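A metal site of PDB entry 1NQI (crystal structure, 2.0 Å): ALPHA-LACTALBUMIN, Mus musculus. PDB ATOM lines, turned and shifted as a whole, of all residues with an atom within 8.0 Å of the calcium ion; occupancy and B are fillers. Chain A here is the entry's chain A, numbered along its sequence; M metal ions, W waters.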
ATOM      1  N   THR A  38      13.760  12.749  -1.115  1.00  0.00           N
ATOM      2  CA  THR A  38      14.904  11.840  -1.153  1.00  0.00           C
ATOM      3  C   THR A  38      14.603  10.524  -1.884  1.00  0.00           C
ATOM      4  O   THR A  38      15.538   9.804  -2.246  1.00  0.00           O
ATOM      5  CB  THR A  38      15.407  11.461   0.253  1.00  0.00           C
ATOM      6  OG1 THR A  38      14.358  10.820   0.984  1.00  0.00           O
ATOM      7  CG2 THR A  38      15.880  12.701   1.003  1.00  0.00           C
ATOM      8  N   GLY A  51      16.513   9.963  -6.485  1.00  0.00           N
ATOM      9  CA  GLY A  51      16.688  10.823  -5.331  1.00  0.00           C
ATOM     10  C   GLY A  51      16.648  12.337  -5.462  1.00  0.00           C
ATOM     11  O   GLY A  51      16.212  12.916  -6.477  1.00  0.00           O
ATOM     12  N   ILE A  75      28.297   3.272  -7.109  1.00  0.00           N
ATOM     13  CA  ILE A  75      27.289   3.107  -6.079  1.00  0.00           C
ATOM     14  C   ILE A  75      26.049   2.531  -6.721  1.00  0.00           C
ATOM     15  O   ILE A  75      25.773   2.791  -7.889  1.00  0.00           O
ATOM     16  CB  ILE A  75      26.919   4.493  -5.493  1.00  0.00           C
ATOM     17  CG1 ILE A  75      25.935   4.365  -4.349  1.00  0.00           C
ATOM     18  CG2 ILE A  75      26.264   5.338  -6.585  1.00  0.00           C
ATOM     19  CD1 ILE A  75      25.428   5.743  -3.823  1.00  0.00           C
ATOM     20  N   SER A  76      25.286   1.778  -5.949  1.00  0.00           N
ATOM     21  CA  SER A  76      24.050   1.218  -6.435  1.00  0.00           C
ATOM     22  C   SER A  76      23.042   2.382  -6.426  1.00  0.00           C
ATOM     23  O   SER A  76      23.056   3.162  -5.473  1.00  0.00           O
ATOM     24  CB  SER A  76      23.583   0.114  -5.492  1.00  0.00           C
ATOM     25  OG  SER A  76      22.256  -0.204  -5.810  1.00  0.00           O
ATOM     26  N   CYS A  77      22.211   2.515  -7.451  1.00  0.00           N
ATOM     27  CA  CYS A  77      21.243   3.620  -7.516  1.00  0.00           C
ATOM     28  C   CYS A  77      20.299   3.646  -6.291  1.00  0.00           C
ATOM     29  O   CYS A  77      19.791   4.707  -5.912  1.00  0.00           O
ATOM     30  CB  CYS A  77      20.408   3.568  -8.797  1.00  0.00           C
ATOM     31  SG  CYS A  77      21.323   3.689 -10.402  1.00  0.00           S
ATOM     32  N   ASP A  78      20.029   2.489  -5.697  1.00  0.00           N
ATOM     33  CA  ASP A  78      19.164   2.447  -4.530  1.00  0.00           C
ATOM     34  C   ASP A  78      19.764   3.170  -3.300  1.00  0.00           C
ATOM     35  O   ASP A  78      19.025   3.545  -2.404  1.00  0.00           O
ATOM     36  CB  ASP A  78      18.787   1.003  -4.197  1.00  0.00           C
ATOM     37  CG  ASP A  78      18.012   0.342  -5.329  1.00  0.00           C
ATOM     38  OD1 ASP A  78      17.099   1.004  -5.880  1.00  0.00           O
ATOM     39  OD2 ASP A  78      18.303  -0.829  -5.676  1.00  0.00           O
ATOM     40  N   LYS A  79      21.070   3.395  -3.256  1.00  0.00           N
ATOM     41  CA  LYS A  79      21.671   4.129  -2.134  1.00  0.00           C
ATOM     42  C   LYS A  79      21.310   5.624  -2.275  1.00  0.00           C
ATOM     43  O   LYS A  79      21.613   6.433  -1.384  1.00  0.00           O
ATOM     44  CB  LYS A  79      23.196   4.010  -2.118  1.00  0.00           C
ATOM     45  CG  LYS A  79      23.719   2.628  -1.692  1.00  0.00           C
ATOM     46  CD  LYS A  79      23.354   2.402  -0.260  1.00  0.00           C
ATOM     47  CE  LYS A  79      24.141   1.291   0.367  1.00  0.00           C
ATOM     48  NZ  LYS A  79      24.002   1.309   1.855  1.00  0.00           N
ATOM     49  N   LEU A  80      20.679   5.960  -3.382  1.00  0.00           N
ATOM     50  CA  LEU A  80      20.266   7.343  -3.689  1.00  0.00           C
ATOM     51  C   LEU A  80      18.794   7.560  -3.365  1.00  0.00           C
ATOM     52  O   LEU A  80      18.226   8.611  -3.684  1.00  0.00           O
ATOM     53  CB  LEU A  80      20.521   7.636  -5.163  1.00  0.00           C
ATOM     54  CG  LEU A  80      22.013   7.584  -5.553  1.00  0.00           C
ATOM     55  CD1 LEU A  80      22.140   7.906  -7.067  1.00  0.00           C
ATOM     56  CD2 LEU A  80      22.833   8.608  -4.716  1.00  0.00           C
ATOM     57  N   LEU A  81      18.192   6.575  -2.717  1.00  0.00           N
ATOM     58  CA  LEU A  81      16.793   6.680  -2.348  1.00  0.00           C
ATOM     59  C   LEU A  81      16.548   6.639  -0.834  1.00  0.00           C
ATOM     60  O   LEU A  81      15.443   6.311  -0.390  1.00  0.00           O
ATOM     61  CB  LEU A  81      15.975   5.570  -3.054  1.00  0.00           C
ATOM     62  CG  LEU A  81      15.916   5.669  -4.593  1.00  0.00           C
ATOM     63  CD1 LEU A  81      15.264   4.429  -5.206  1.00  0.00           C
ATOM     64  CD2 LEU A  81      15.170   6.921  -4.998  1.00  0.00           C
ATOM     65  N   ASP A  82      17.545   6.977  -0.024  1.00  0.00           N
ATOM     66  CA  ASP A  82      17.355   7.013   1.415  1.00  0.00           C
ATOM     67  C   ASP A  82      17.586   8.421   1.957  1.00  0.00           C
ATOM     68  O   ASP A  82      17.724   9.386   1.184  1.00  0.00           O
ATOM     69  CB  ASP A  82      18.303   6.018   2.125  1.00  0.00           C
ATOM     70  CG  ASP A  82      19.767   6.240   1.754  1.00  0.00           C
ATOM     71  OD1 ASP A  82      20.216   7.400   1.782  1.00  0.00           O
ATOM     72  OD2 ASP A  82      20.456   5.238   1.448  1.00  0.00           O
ATOM     73  N   ASP A  83      17.610   8.556   3.279  1.00  0.00           N
ATOM     74  CA  ASP A  83      17.821   9.851   3.899  1.00  0.00           C
ATOM     75  C   ASP A  83      19.279  10.129   4.287  1.00  0.00           C
ATOM     76  O   ASP A  83      19.567  11.113   4.984  1.00  0.00           O
ATOM     77  CB  ASP A  83      16.887  10.008   5.108  1.00  0.00           C
ATOM     78  CG  ASP A  83      15.426  10.096   4.686  1.00  0.00           C
ATOM     79  OD1 ASP A  83      15.157  10.259   3.463  1.00  0.00           O
ATOM     80  OD2 ASP A  83      14.546  10.024   5.565  1.00  0.00           O
ATOM     81  N   GLU A  84      20.194   9.302   3.824  1.00  0.00           N
ATOM     82  CA  GLU A  84      21.607   9.523   4.106  1.00  0.00           C
ATOM     83  C   GLU A  84      22.172  10.094   2.816  1.00  0.00           C
ATOM     84  O   GLU A  84      22.400   9.399   1.827  1.00  0.00           O
ATOM     85  CB  GLU A  84      22.299   8.239   4.529  1.00  0.00           C
ATOM     86  CG  GLU A  84      21.920   7.791   5.956  1.00  0.00           C
ATOM     87  CD  GLU A  84      22.067   6.268   6.120  1.00  0.00           C
ATOM     88  OE1 GLU A  84      21.067   5.618   6.521  1.00  0.00           O
ATOM     89  OE2 GLU A  84      23.163   5.729   5.847  1.00  0.00           O
ATOM     90  N   LEU A  85      22.365  11.406   2.863  1.00  0.00           N
ATOM     91  CA  LEU A  85      22.800  12.176   1.712  1.00  0.00           C
ATOM     92  C   LEU A  85      24.273  12.243   1.373  1.00  0.00           C
ATOM     93  O   LEU A  85      24.631  12.800   0.319  1.00  0.00           O
ATOM     94  CB  LEU A  85      22.238  13.595   1.882  1.00  0.00           C
ATOM     95  CG  LEU A  85      20.773  13.803   1.492  1.00  0.00           C
ATOM     96  CD1 LEU A  85      19.969  12.539   1.531  1.00  0.00           C
ATOM     97  CD2 LEU A  85      20.180  14.880   2.354  1.00  0.00           C
ATOM     98  N   ASP A  86      25.119  11.703   2.235  1.00  0.00           N
ATOM     99  CA  ASP A  86      26.564  11.743   2.001  1.00  0.00           C
ATOM    100  C   ASP A  86      26.971  11.172   0.650  1.00  0.00           C
ATOM    101  O   ASP A  86      27.710  11.798  -0.097  1.00  0.00           O
ATOM    102  CB  ASP A  86      27.339  11.048   3.124  1.00  0.00           C
ATOM    103  CG  ASP A  86      27.208  11.791   4.465  1.00  0.00           C
ATOM    104  OD1 ASP A  86      26.135  11.695   5.093  1.00  0.00           O
ATOM    105  OD2 ASP A  86      28.187  12.456   4.891  1.00  0.00           O
ATOM    106  N   ASP A  87      26.458   9.984   0.322  1.00  0.00           N
ATOM    107  CA  ASP A  87      26.853   9.399  -0.948  1.00  0.00           C
ATOM    108  C   ASP A  87      26.180  10.100  -2.134  1.00  0.00           C
ATOM    109  O   ASP A  87      26.758  10.150  -3.222  1.00  0.00           O
ATOM    110  CB  ASP A  87      26.606   7.868  -0.975  1.00  0.00           C
ATOM    111  CG  ASP A  87      25.157   7.440  -0.605  1.00  0.00           C
ATOM    112  OD1 ASP A  87      24.232   8.259  -0.454  1.00  0.00           O
ATOM    113  OD2 ASP A  87      24.965   6.204  -0.481  1.00  0.00           O
ATOM    114  N   ASP A  88      24.981  10.659  -1.945  1.00  0.00           N
ATOM    115  CA  ASP A  88      24.322  11.372  -3.042  1.00  0.00           C
ATOM    116  C   ASP A  88      25.164  12.582  -3.391  1.00  0.00           C
ATOM    117  O   ASP A  88      25.395  12.911  -4.559  1.00  0.00           O
ATOM    118  CB  ASP A  88      22.930  11.887  -2.616  1.00  0.00           C
ATOM    119  CG  ASP A  88      22.012  10.779  -2.126  1.00  0.00           C
ATOM    120  OD1 ASP A  88      20.910  10.638  -2.667  1.00  0.00           O
ATOM    121  OD2 ASP A  88      22.388  10.056  -1.204  1.00  0.00           O
ATOM    122  N   ILE A  89      25.605  13.276  -2.349  1.00  0.00           N
ATOM    123  CA  ILE A  89      26.402  14.500  -2.487  1.00  0.00           C
ATOM    124  C   ILE A  89      27.753  14.186  -3.136  1.00  0.00           C
ATOM    125  O   ILE A  89      28.215  14.931  -3.986  1.00  0.00           O
ATOM    126  CB  ILE A  89      26.621  15.150  -1.115  1.00  0.00           C
ATOM    127  CG1 ILE A  89      25.243  15.543  -0.515  1.00  0.00           C
ATOM    128  CG2 ILE A  89      27.555  16.372  -1.220  1.00  0.00           C
ATOM    129  CD1 ILE A  89      25.294  15.950   0.918  1.00  0.00           C
HETATM  130 CA    CA M   1      21.936   8.136   0.018  1.00  0.00          CA
HETATM  131  O   HOH W   1      19.674   9.005  -0.714  1.00  0.00           O
HETATM  132  O   HOH W   2      22.931   6.270   1.409  1.00  0.00           O
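Along chain A the residues within 4 Å of the calcium ion span positions 79 to 88.
The calcium ion is bound by the backbone carbonyl oxygen of Lys 79 (2.2 Å), the backbone carbonyl oxygen of Glu 84 (2.3 Å), the side-chain carboxylate of Asp 88 (2.3 Å), the side-chain carboxylate of Asp 87 (2.3 Å), water W2 (2.5 Å), water W1 (2.5 Å) and the side-chain carboxylate of Asp 82 (2.6 Å).
Water W2 lies within hydrogen-bond range of OD2 of Asp 82 (2.7 Å) and OD2 of Asp 87 (2.8 Å).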
